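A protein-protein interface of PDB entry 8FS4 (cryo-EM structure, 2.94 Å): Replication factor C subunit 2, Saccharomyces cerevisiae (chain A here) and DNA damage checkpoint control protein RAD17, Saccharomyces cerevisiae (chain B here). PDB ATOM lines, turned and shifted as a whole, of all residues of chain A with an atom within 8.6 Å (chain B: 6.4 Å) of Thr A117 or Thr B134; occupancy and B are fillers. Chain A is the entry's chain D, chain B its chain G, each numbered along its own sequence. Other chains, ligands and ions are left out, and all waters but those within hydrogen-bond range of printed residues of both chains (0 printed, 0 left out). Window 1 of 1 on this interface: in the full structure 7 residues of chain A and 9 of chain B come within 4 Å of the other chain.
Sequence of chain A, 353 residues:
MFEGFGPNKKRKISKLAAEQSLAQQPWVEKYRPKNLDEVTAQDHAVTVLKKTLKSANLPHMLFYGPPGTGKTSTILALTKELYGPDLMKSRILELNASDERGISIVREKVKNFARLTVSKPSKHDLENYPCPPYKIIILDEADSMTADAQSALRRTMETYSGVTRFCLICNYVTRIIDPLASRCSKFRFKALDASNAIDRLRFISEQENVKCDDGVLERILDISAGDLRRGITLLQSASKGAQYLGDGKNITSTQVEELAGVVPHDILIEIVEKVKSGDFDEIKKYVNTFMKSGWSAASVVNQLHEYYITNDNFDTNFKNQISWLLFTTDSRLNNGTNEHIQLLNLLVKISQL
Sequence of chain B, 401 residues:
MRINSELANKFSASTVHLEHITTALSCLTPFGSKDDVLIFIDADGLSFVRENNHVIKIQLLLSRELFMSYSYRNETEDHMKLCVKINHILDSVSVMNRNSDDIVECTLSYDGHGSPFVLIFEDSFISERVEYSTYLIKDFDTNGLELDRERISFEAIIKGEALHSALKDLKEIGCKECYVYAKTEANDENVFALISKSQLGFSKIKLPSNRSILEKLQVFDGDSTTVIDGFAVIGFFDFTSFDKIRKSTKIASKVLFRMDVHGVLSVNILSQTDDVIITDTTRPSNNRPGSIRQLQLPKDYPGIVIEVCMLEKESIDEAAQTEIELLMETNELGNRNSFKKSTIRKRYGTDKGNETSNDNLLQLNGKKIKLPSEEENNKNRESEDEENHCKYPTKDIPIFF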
ATOM      1  N   SER A  90     -10.825  33.348  -6.316  1.00  0.00           N
ATOM      2  CA  SER A  90      -9.574  32.666  -6.611  1.00  0.00           C
ATOM      3  C   SER A  90      -9.740  31.428  -7.477  1.00  0.00           C
ATOM      4  O   SER A  90      -8.776  31.031  -8.138  1.00  0.00           O
ATOM      5  CB  SER A  90      -8.871  32.263  -5.307  1.00  0.00           C
ATOM      6  OG  SER A  90      -9.643  31.323  -4.582  1.00  0.00           O
ATOM      7  N   ARG A  91     -10.921  30.810  -7.498  1.00  0.00           N
ATOM      8  CA  ARG A  91     -11.131  29.574  -8.239  1.00  0.00           C
ATOM      9  C   ARG A  91     -12.053  29.740  -9.441  1.00  0.00           C
ATOM     10  O   ARG A  91     -12.541  28.738  -9.969  1.00  0.00           O
ATOM     11  CB  ARG A  91     -11.695  28.496  -7.315  1.00  0.00           C
ATOM     12  CG  ARG A  91     -10.765  28.100  -6.188  1.00  0.00           C
ATOM     13  CD  ARG A  91      -9.943  26.877  -6.527  1.00  0.00           C
ATOM     14  NE  ARG A  91     -10.534  25.667  -5.969  1.00  0.00           N
ATOM     15  CZ  ARG A  91     -10.302  25.212  -4.746  1.00  0.00           C
ATOM     16  NH1 ARG A  91      -9.490  25.843  -3.915  1.00  0.00           N
ATOM     17  NH2 ARG A  91     -10.901  24.095  -4.345  1.00  0.00           N
ATOM     18  N   ASN A 112      -2.211  30.118 -18.568  1.00  0.00           N
ATOM     19  CA  ASN A 112      -1.602  30.353 -17.266  1.00  0.00           C
ATOM     20  C   ASN A 112      -2.592  30.096 -16.142  1.00  0.00           C
ATOM     21  O   ASN A 112      -2.223  29.539 -15.102  1.00  0.00           O
ATOM     22  CB  ASN A 112      -1.064  31.780 -17.191  1.00  0.00           C
ATOM     23  CG  ASN A 112       0.213  31.963 -17.985  1.00  0.00           C
ATOM     24  OD1 ASN A 112       0.855  30.991 -18.382  1.00  0.00           O
ATOM     25  ND2 ASN A 112       0.591  33.213 -18.221  1.00  0.00           N
ATOM     26  N   PHE A 113      -3.853  30.493 -16.319  1.00  0.00           N
ATOM     27  CA  PHE A 113      -4.839  30.214 -15.281  1.00  0.00           C
ATOM     28  C   PHE A 113      -5.101  28.720 -15.154  1.00  0.00           C
ATOM     29  O   PHE A 113      -5.303  28.212 -14.045  1.00  0.00           O
ATOM     30  CB  PHE A 113      -6.145  30.954 -15.556  1.00  0.00           C
ATOM     31  CG  PHE A 113      -7.109  30.899 -14.408  1.00  0.00           C
ATOM     32  CD1 PHE A 113      -7.016  31.802 -13.367  1.00  0.00           C
ATOM     33  CD2 PHE A 113      -8.094  29.932 -14.360  1.00  0.00           C
ATOM     34  CE1 PHE A 113      -7.891  31.747 -12.309  1.00  0.00           C
ATOM     35  CE2 PHE A 113      -8.972  29.875 -13.303  1.00  0.00           C
ATOM     36  CZ  PHE A 113      -8.868  30.782 -12.277  1.00  0.00           C
ATOM     37  N   ALA A 114      -5.117  27.996 -16.274  1.00  0.00           N
ATOM     38  CA  ALA A 114      -5.284  26.551 -16.201  1.00  0.00           C
ATOM     39  C   ALA A 114      -4.089  25.893 -15.529  1.00  0.00           C
ATOM     40  O   ALA A 114      -4.250  24.906 -14.802  1.00  0.00           O
ATOM     41  CB  ALA A 114      -5.492  25.975 -17.600  1.00  0.00           C
ATOM     42  N   ARG A 115      -2.887  26.427 -15.754  1.00  0.00           N
ATOM     43  CA  ARG A 115      -1.671  25.897 -15.153  1.00  0.00           C
ATOM     44  C   ARG A 115      -1.551  26.228 -13.674  1.00  0.00           C
ATOM     45  O   ARG A 115      -0.704  25.642 -12.995  1.00  0.00           O
ATOM     46  CB  ARG A 115      -0.451  26.443 -15.894  1.00  0.00           C
ATOM     47  CG  ARG A 115       0.377  25.379 -16.563  1.00  0.00           C
ATOM     48  CD  ARG A 115       1.669  25.942 -17.136  1.00  0.00           C
ATOM     49  NE  ARG A 115       2.789  25.856 -16.205  1.00  0.00           N
ATOM     50  CZ  ARG A 115       3.270  24.728 -15.699  1.00  0.00           C
ATOM     51  NH1 ARG A 115       2.746  23.551 -16.004  1.00  0.00           N
ATOM     52  NH2 ARG A 115       4.301  24.782 -14.862  1.00  0.00           N
ATOM     53  N   LEU A 116      -2.368  27.142 -13.163  1.00  0.00           N
ATOM     54  CA  LEU A 116      -2.270  27.547 -11.772  1.00  0.00           C
ATOM     55  C   LEU A 116      -2.619  26.391 -10.843  1.00  0.00           C
ATOM     56  O   LEU A 116      -3.377  25.485 -11.195  1.00  0.00           O
ATOM     57  CB  LEU A 116      -3.206  28.719 -11.490  1.00  0.00           C
ATOM     58  CG  LEU A 116      -2.568  30.097 -11.357  1.00  0.00           C
ATOM     59  CD1 LEU A 116      -3.646  31.158 -11.252  1.00  0.00           C
ATOM     60  CD2 LEU A 116      -1.654  30.151 -10.159  1.00  0.00           C
ATOM     61  N   THR A 117      -2.053  26.433  -9.642  1.00  0.00           N
ATOM     62  CA  THR A 117      -2.371  25.446  -8.627  1.00  0.00           C
ATOM     63  C   THR A 117      -3.677  25.800  -7.931  1.00  0.00           C
ATOM     64  O   THR A 117      -4.020  26.974  -7.761  1.00  0.00           O
ATOM     65  CB  THR A 117      -1.253  25.352  -7.591  1.00  0.00           C
ATOM     66  OG1 THR A 117       0.013  25.571  -8.225  1.00  0.00           O
ATOM     67  CG2 THR A 117      -1.262  23.982  -6.932  1.00  0.00           C
ATOM     68  N   VAL A 118      -4.407  24.766  -7.523  1.00  0.00           N
ATOM     69  CA  VAL A 118      -5.658  24.965  -6.804  1.00  0.00           C
ATOM     70  C   VAL A 118      -5.345  25.590  -5.451  1.00  0.00           C
ATOM     71  O   VAL A 118      -4.565  25.043  -4.663  1.00  0.00           O
ATOM     72  CB  VAL A 118      -6.411  23.639  -6.651  1.00  0.00           C
ATOM     73  CG1 VAL A 118      -7.318  23.668  -5.434  1.00  0.00           C
ATOM     74  CG2 VAL A 118      -7.210  23.345  -7.901  1.00  0.00           C
ATOM     75  N   SER A 119      -5.957  26.737  -5.175  1.00  0.00           N
ATOM     76  CA  SER A 119      -5.719  27.433  -3.920  1.00  0.00           C
ATOM     77  C   SER A 119      -6.268  26.629  -2.748  1.00  0.00           C
ATOM     78  O   SER A 119      -7.232  25.870  -2.882  1.00  0.00           O
ATOM     79  CB  SER A 119      -6.360  28.818  -3.950  1.00  0.00           C
ATOM     80  OG  SER A 119      -5.541  29.739  -4.647  1.00  0.00           O
ATOM     81  N   LYS A 120      -5.646  26.803  -1.592  1.00  0.00           N
ATOM     82  CA  LYS A 120      -6.050  26.063  -0.404  1.00  0.00           C
ATOM     83  C   LYS A 120      -7.356  26.634   0.135  1.00  0.00           C
ATOM     84  O   LYS A 120      -7.403  27.823   0.476  1.00  0.00           O
ATOM     85  CB  LYS A 120      -4.959  26.137   0.658  1.00  0.00           C
ATOM     86  CG  LYS A 120      -4.895  24.924   1.578  1.00  0.00           C
ATOM     87  CD  LYS A 120      -5.590  25.191   2.903  1.00  0.00           C
ATOM     88  CE  LYS A 120      -6.100  23.907   3.535  1.00  0.00           C
ATOM     89  NZ  LYS A 120      -6.866  24.164   4.785  1.00  0.00           N
ATOM     90  N   PRO A 133     -11.614  20.039  -5.885  1.00  0.00           N
ATOM     91  CA  PRO A 133     -10.187  20.304  -6.101  1.00  0.00           C
ATOM     92  C   PRO A 133      -9.842  20.737  -7.526  1.00  0.00           C
ATOM     93  O   PRO A 133      -8.886  20.249  -8.129  1.00  0.00           O
ATOM     94  CB  PRO A 133      -9.542  18.960  -5.751  1.00  0.00           C
ATOM     95  CG  PRO A 133     -10.564  17.963  -6.135  1.00  0.00           C
ATOM     96  CD  PRO A 133     -11.899  18.594  -5.847  1.00  0.00           C
ATOM     97  N   TYR A 134     -10.622  21.670  -8.065  1.00  0.00           N
ATOM     98  CA  TYR A 134     -10.349  22.209  -9.389  1.00  0.00           C
ATOM     99  C   TYR A 134     -11.010  23.572  -9.504  1.00  0.00           C
ATOM    100  O   TYR A 134     -11.865  23.940  -8.697  1.00  0.00           O
ATOM    101  CB  TYR A 134     -10.844  21.278 -10.503  1.00  0.00           C
ATOM    102  CG  TYR A 134     -12.241  20.745 -10.301  1.00  0.00           C
ATOM    103  CD1 TYR A 134     -13.350  21.539 -10.537  1.00  0.00           C
ATOM    104  CD2 TYR A 134     -12.451  19.439  -9.887  1.00  0.00           C
ATOM    105  CE1 TYR A 134     -14.626  21.053 -10.357  1.00  0.00           C
ATOM    106  CE2 TYR A 134     -13.723  18.944  -9.706  1.00  0.00           C
ATOM    107  CZ  TYR A 134     -14.806  19.755  -9.942  1.00  0.00           C
ATOM    108  OH  TYR A 134     -16.076  19.264  -9.762  1.00  0.00           O
ATOM    109  N   LYS A 135     -10.597  24.316 -10.522  1.00  0.00           N
ATOM    110  CA  LYS A 135     -11.174  25.611 -10.840  1.00  0.00           C
ATOM    111  C   LYS A 135     -11.959  25.511 -12.139  1.00  0.00           C
ATOM    112  O   LYS A 135     -11.809  24.558 -12.907  1.00  0.00           O
ATOM    113  CB  LYS A 135     -10.091  26.687 -10.954  1.00  0.00           C
ATOM    114  CG  LYS A 135      -8.693  26.149 -11.165  1.00  0.00           C
ATOM    115  CD  LYS A 135      -7.709  27.274 -11.396  1.00  0.00           C
ATOM    116  CE  LYS A 135      -6.281  26.774 -11.422  1.00  0.00           C
ATOM    117  NZ  LYS A 135      -6.101  25.666 -12.389  1.00  0.00           N
ATOM    118  N   VAL A 163      -7.096  19.706 -13.016  1.00  0.00           N
ATOM    119  CA  VAL A 163      -6.888  20.824 -12.102  1.00  0.00           C
ATOM    120  C   VAL A 163      -7.709  22.028 -12.544  1.00  0.00           C
ATOM    121  O   VAL A 163      -7.769  23.039 -11.838  1.00  0.00           O
ATOM    122  CB  VAL A 163      -5.395  21.186 -12.007  1.00  0.00           C
ATOM    123  CG1 VAL A 163      -4.981  22.099 -13.153  1.00  0.00           C
ATOM    124  CG2 VAL A 163      -5.095  21.837 -10.677  1.00  0.00           C
ATOM    125  N   THR A 164      -8.339  21.935 -13.714  1.00  0.00           N
ATOM    126  CA  THR A 164      -9.083  23.054 -14.273  1.00  0.00           C
ATOM    127  C   THR A 164     -10.206  22.510 -15.138  1.00  0.00           C
ATOM    128  O   THR A 164      -9.996  21.565 -15.904  1.00  0.00           O
ATOM    129  CB  THR A 164      -8.167  23.964 -15.098  1.00  0.00           C
ATOM    130  OG1 THR A 164      -7.287  24.673 -14.221  1.00  0.00           O
ATOM    131  CG2 THR A 164      -8.969  24.965 -15.913  1.00  0.00           C
ATOM    132  N   LYS B  81       8.416  20.722  -3.867  1.00  0.00           N
ATOM    133  CA  LYS B  81       8.593  21.259  -5.208  1.00  0.00           C
ATOM    134  C   LYS B  81       7.492  22.268  -5.498  1.00  0.00           C
ATOM    135  O   LYS B  81       6.315  22.001  -5.232  1.00  0.00           O
ATOM    136  CB  LYS B  81       8.559  20.144  -6.256  1.00  0.00           C
ATOM    137  CG  LYS B  81       9.676  19.123  -6.121  1.00  0.00           C
ATOM    138  CD  LYS B  81       9.324  17.782  -6.762  1.00  0.00           C
ATOM    139  CE  LYS B  81       8.697  17.929  -8.145  1.00  0.00           C
ATOM    140  NZ  LYS B  81       9.648  18.495  -9.139  1.00  0.00           N
ATOM    141  N   LEU B  82       7.874  23.422  -6.038  1.00  0.00           N
ATOM    142  CA  LEU B  82       6.918  24.431  -6.466  1.00  0.00           C
ATOM    143  C   LEU B  82       7.414  25.073  -7.752  1.00  0.00           C
ATOM    144  O   LEU B  82       8.620  25.179  -7.986  1.00  0.00           O
ATOM    145  CB  LEU B  82       6.703  25.505  -5.394  1.00  0.00           C
ATOM    146  CG  LEU B  82       7.960  26.225  -4.911  1.00  0.00           C
ATOM    147  CD1 LEU B  82       7.666  27.694  -4.686  1.00  0.00           C
ATOM    148  CD2 LEU B  82       8.487  25.581  -3.642  1.00  0.00           C
ATOM    149  N   CYS B  83       6.469  25.510  -8.581  1.00  0.00           N
ATOM    150  CA  CYS B  83       6.769  26.118  -9.873  1.00  0.00           C
ATOM    151  C   CYS B  83       6.186  27.521  -9.893  1.00  0.00           C
ATOM    152  O   CYS B  83       4.970  27.693  -9.765  1.00  0.00           O
ATOM    153  CB  CYS B  83       6.203  25.280 -11.017  1.00  0.00           C
ATOM    154  SG  CYS B  83       7.428  24.279 -11.866  1.00  0.00           S
ATOM    155  N   VAL B  84       7.047  28.518 -10.059  1.00  0.00           N
ATOM    156  CA  VAL B  84       6.628  29.909 -10.142  1.00  0.00           C
ATOM    157  C   VAL B  84       7.303  30.543 -11.348  1.00  0.00           C
ATOM    158  O   VAL B  84       8.406  30.151 -11.744  1.00  0.00           O
ATOM    159  CB  VAL B  84       6.964  30.693  -8.855  1.00  0.00           C
ATOM    160  CG1 VAL B  84       6.331  30.025  -7.647  1.00  0.00           C
ATOM    161  CG2 VAL B  84       8.465  30.805  -8.673  1.00  0.00           C
ATOM    162  N   TYR B 110       6.860  29.330   2.471  1.00  0.00           N
ATOM    163  CA  TYR B 110       6.021  28.460   1.652  1.00  0.00           C
ATOM    164  C   TYR B 110       5.251  27.544   2.586  1.00  0.00           C
ATOM    165  O   TYR B 110       5.861  26.850   3.405  1.00  0.00           O
ATOM    166  CB  TYR B 110       6.864  27.649   0.672  1.00  0.00           C
ATOM    167  CG  TYR B 110       6.052  26.904  -0.361  1.00  0.00           C
ATOM    168  CD1 TYR B 110       5.275  27.585  -1.285  1.00  0.00           C
ATOM    169  CD2 TYR B 110       6.064  25.520  -0.413  1.00  0.00           C
ATOM    170  CE1 TYR B 110       4.532  26.911  -2.228  1.00  0.00           C
ATOM    171  CE2 TYR B 110       5.324  24.836  -1.354  1.00  0.00           C
ATOM    172  CZ  TYR B 110       4.561  25.538  -2.259  1.00  0.00           C
ATOM    173  OH  TYR B 110       3.822  24.863  -3.201  1.00  0.00           O
ATOM    174  N   GLY B 112       3.094  25.047   1.682  1.00  0.00           N
ATOM    175  CA  GLY B 112       2.751  23.768   1.093  1.00  0.00           C
ATOM    176  C   GLY B 112       2.043  23.940  -0.234  1.00  0.00           C
ATOM    177  O   GLY B 112       1.939  25.040  -0.781  1.00  0.00           O
ATOM    178  N   HIS B 113       1.544  22.821  -0.755  1.00  0.00           N
ATOM    179  CA  HIS B 113       0.870  22.836  -2.046  1.00  0.00           C
ATOM    180  C   HIS B 113      -0.397  23.677  -1.969  1.00  0.00           C
ATOM    181  O   HIS B 113      -1.169  23.573  -1.011  1.00  0.00           O
ATOM    182  CB  HIS B 113       0.532  21.414  -2.487  1.00  0.00           C
ATOM    183  CG  HIS B 113       0.388  21.261  -3.969  1.00  0.00           C
ATOM    184  ND1 HIS B 113       1.285  21.801  -4.865  1.00  0.00           N
ATOM    185  CD2 HIS B 113      -0.551  20.629  -4.712  1.00  0.00           C
ATOM    186  CE1 HIS B 113       0.906  21.509  -6.096  1.00  0.00           C
ATOM    187  NE2 HIS B 113      -0.206  20.798  -6.031  1.00  0.00           N
ATOM    188  N   GLY B 114      -0.612  24.509  -2.987  1.00  0.00           N
ATOM    189  CA  GLY B 114      -1.755  25.389  -3.038  1.00  0.00           C
ATOM    190  C   GLY B 114      -1.539  26.741  -2.397  1.00  0.00           C
ATOM    191  O   GLY B 114      -2.408  27.613  -2.525  1.00  0.00           O
ATOM    192  N   SER B 115      -0.419  26.945  -1.721  1.00  0.00           N
ATOM    193  CA  SER B 115      -0.130  28.211  -1.075  1.00  0.00           C
ATOM    194  C   SER B 115       0.919  28.985  -1.864  1.00  0.00           C
ATOM    195  O   SER B 115       1.803  28.388  -2.484  1.00  0.00           O
ATOM    196  CB  SER B 115       0.369  27.976   0.352  1.00  0.00           C
ATOM    197  OG  SER B 115      -0.602  27.267   1.103  1.00  0.00           O
ATOM    198  N   PRO B 116       0.853  30.311  -1.870  1.00  0.00           N
ATOM    199  CA  PRO B 116       1.800  31.094  -2.667  1.00  0.00           C
ATOM    200  C   PRO B 116       3.179  31.146  -2.029  1.00  0.00           C
ATOM    201  O   PRO B 116       3.366  30.869  -0.843  1.00  0.00           O
ATOM    202  CB  PRO B 116       1.160  32.483  -2.704  1.00  0.00           C
ATOM    203  CG  PRO B 116       0.398  32.564  -1.434  1.00  0.00           C
ATOM    204  CD  PRO B 116      -0.102  31.173  -1.151  1.00  0.00           C
ATOM    205  N   PHE B 117       4.156  31.515  -2.852  1.00  0.00           N
ATOM    206  CA  PHE B 117       5.527  31.707  -2.399  1.00  0.00           C
ATOM    207  C   PHE B 117       5.687  33.144  -1.918  1.00  0.00           C
ATOM    208  O   PHE B 117       5.574  34.085  -2.710  1.00  0.00           O
ATOM    209  CB  PHE B 117       6.508  31.399  -3.527  1.00  0.00           C
ATOM    210  CG  PHE B 117       7.919  31.190  -3.065  1.00  0.00           C
ATOM    211  CD1 PHE B 117       8.226  30.191  -2.157  1.00  0.00           C
ATOM    212  CD2 PHE B 117       8.942  31.995  -3.539  1.00  0.00           C
ATOM    213  CE1 PHE B 117       9.523  30.000  -1.732  1.00  0.00           C
ATOM    214  CE2 PHE B 117      10.241  31.809  -3.116  1.00  0.00           C
ATOM    215  CZ  PHE B 117      10.531  30.810  -2.211  1.00  0.00           C
ATOM    216  N   TYR B 132       3.765  34.997  -4.513  1.00  0.00           N
ATOM    217  CA  TYR B 132       3.880  34.563  -5.897  1.00  0.00           C
ATOM    218  C   TYR B 132       3.001  33.343  -6.124  1.00  0.00           C
ATOM    219  O   TYR B 132       3.050  32.381  -5.351  1.00  0.00           O
ATOM    220  CB  TYR B 132       5.331  34.235  -6.248  1.00  0.00           C
ATOM    221  CG  TYR B 132       6.275  35.406  -6.132  1.00  0.00           C
ATOM    222  CD1 TYR B 132       6.282  36.414  -7.086  1.00  0.00           C
ATOM    223  CD2 TYR B 132       7.162  35.501  -5.072  1.00  0.00           C
ATOM    224  CE1 TYR B 132       7.144  37.484  -6.984  1.00  0.00           C
ATOM    225  CE2 TYR B 132       8.027  36.566  -4.963  1.00  0.00           C
ATOM    226  CZ  TYR B 132       8.015  37.554  -5.921  1.00  0.00           C
ATOM    227  OH  TYR B 132       8.877  38.619  -5.814  1.00  0.00           O
ATOM    228  N   SER B 133       2.199  33.388  -7.182  1.00  0.00           N
ATOM    229  CA  SER B 133       1.300  32.285  -7.488  1.00  0.00           C
ATOM    230  C   SER B 133       2.091  31.085  -7.997  1.00  0.00           C
ATOM    231  O   SER B 133       2.970  31.224  -8.853  1.00  0.00           O
ATOM    232  CB  SER B 133       0.269  32.722  -8.524  1.00  0.00           C
ATOM    233  OG  SER B 133      -0.264  33.997  -8.208  1.00  0.00           O
ATOM    234  N   THR B 134       1.770  29.906  -7.472  1.00  0.00           N
ATOM    235  CA  THR B 134       2.466  28.672  -7.814  1.00  0.00           C
ATOM    236  C   THR B 134       1.680  27.916  -8.875  1.00  0.00           C
ATOM    237  O   THR B 134       0.464  27.735  -8.744  1.00  0.00           O
ATOM    238  CB  THR B 134       2.655  27.796  -6.576  1.00  0.00           C
ATOM    239  OG1 THR B 134       3.399  28.517  -5.589  1.00  0.00           O
ATOM    240  CG2 THR B 134       3.397  26.520  -6.928  1.00  0.00           C
ATOM    241  N   TYR B 135       2.375  27.468  -9.914  1.00  0.00           N
ATOM    242  CA  TYR B 135       1.774  26.766 -11.036  1.00  0.00           C
ATOM    243  C   TYR B 135       2.080  25.278 -10.953  1.00  0.00           C
ATOM    244  O   TYR B 135       2.955  24.833 -10.208  1.00  0.00           O
ATOM    245  CB  TYR B 135       2.276  27.343 -12.364  1.00  0.00           C
ATOM    246  CG  TYR B 135       1.918  28.796 -12.555  1.00  0.00           C
ATOM    247  CD1 TYR B 135       0.714  29.165 -13.138  1.00  0.00           C
ATOM    248  CD2 TYR B 135       2.772  29.800 -12.135  1.00  0.00           C
ATOM    249  CE1 TYR B 135       0.379  30.492 -13.307  1.00  0.00           C
ATOM    250  CE2 TYR B 135       2.442  31.128 -12.295  1.00  0.00           C
ATOM    251  CZ  TYR B 135       1.247  31.469 -12.884  1.00  0.00           C
ATOM    252  OH  TYR B 135       0.919  32.795 -13.047  1.00  0.00           O
ATOM    253  N   LEU B 136       1.330  24.504 -11.732  1.00  0.00           N
ATOM    254  CA  LEU B 136       1.545  23.069 -11.794  1.00  0.00           C
ATOM    255  C   LEU B 136       2.931  22.773 -12.363  1.00  0.00           C
ATOM    256  O   LEU B 136       3.529  23.586 -13.072  1.00  0.00           O
ATOM    257  CB  LEU B 136       0.466  22.406 -12.650  1.00  0.00           C
ATOM    258  CG  LEU B 136      -0.167  21.130 -12.099  1.00  0.00           C
ATOM    259  CD1 LEU B 136      -0.974  21.419 -10.844  1.00  0.00           C
ATOM    260  CD2 LEU B 136      -1.042  20.477 -13.157  1.00  0.00           C
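Among the printed residues, merely in contact across the chains: Asn A112 with Tyr B135, Arg A115 with Tyr B135, Leu A116 with Ser B133, Leu A116 with Thr B134, Leu A116 with Tyr B135, Thr A117 with His B113, Thr A117 with Leu B136, Val A118 with Gly B114 and Ser A119 with Gly B114.
Of the 16 printed residues of chain B, 6 touch a printed residue of chain A.
Printed residues of chain B that touch a printed residue of chain A: His B113, Gly B114, Ser B133, Thr B134, Tyr B135 and Leu B136.
Along chain B the printed residues that touch a printed residue of chain A span positions 113 to 136.
Printed residues of chain A that touch a printed residue of chain B: Asn A112, Arg A115, Leu A116, Thr A117, Val A118, Ser A119 and Lys A120.
Hydrophobic or aromatic side chains of chain A that line the printed part of chain B: Leu A116.
Among the printed residues, 13 pairs touch across the chains.
Of the printed residues of chain B, Asn A112 touches Tyr B135 (3.3 Å).
Of the printed residues of chain B, Thr A117 touches His B113 (3.4 Å), Thr B134 (2.3 Å), Tyr B135 (3.4 Å) and Leu B136 (3.9 Å).
Printed residues of chain B within 4 Å of Val A118: Gly B114 (3.3 Å).
Tyr B110 touches none of the printed residues of chain A.
Tyr B132 touches none of the printed residues of chain A.
Printed residues of chain A within 4 Å of Tyr B135: Asn A112, Arg A115, Leu A116 and Thr A117.
The nearest residue of chain A that does not touch Thr B134 is Arg A115 (4.9 Å).
OG1 of Thr A117 sits close to N of Tyr B135, at 3.5 Å.
The backbone NH (N) of Lys A120 sits at hydrogen-bond distance from the backbone carbonyl oxygen (O) of Gly B114 (3.5 Å).
The backbone NH (N) of Leu B136 lies within hydrogen-bond range of the backbone carbonyl oxygen (O) of Arg A115 (2.7 Å).
The backbone NH of Thr A117 sits at hydrogen-bond distance from the backbone carbonyl oxygen of Thr B134 (3.0 Å).
The backbone carbonyl oxygen (O) of Leu A116 lies within hydrogen-bond range of the side-chain amino group (NZ) of Lys A135 (3.0 Å).
The backbone NH (N) of Tyr B135 sits at hydrogen-bond distance from the backbone carbonyl oxygen (O) of Cys B83 (2.6 Å).
OG1 of Thr B134 lies within hydrogen-bond range of O of Ser B115 (3.5 Å).
The guanidinium group (NH1) of Arg A91 is in hydrogen-bond range of the backbone carbonyl oxygen (O) of Ser A119 (2.5 Å).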
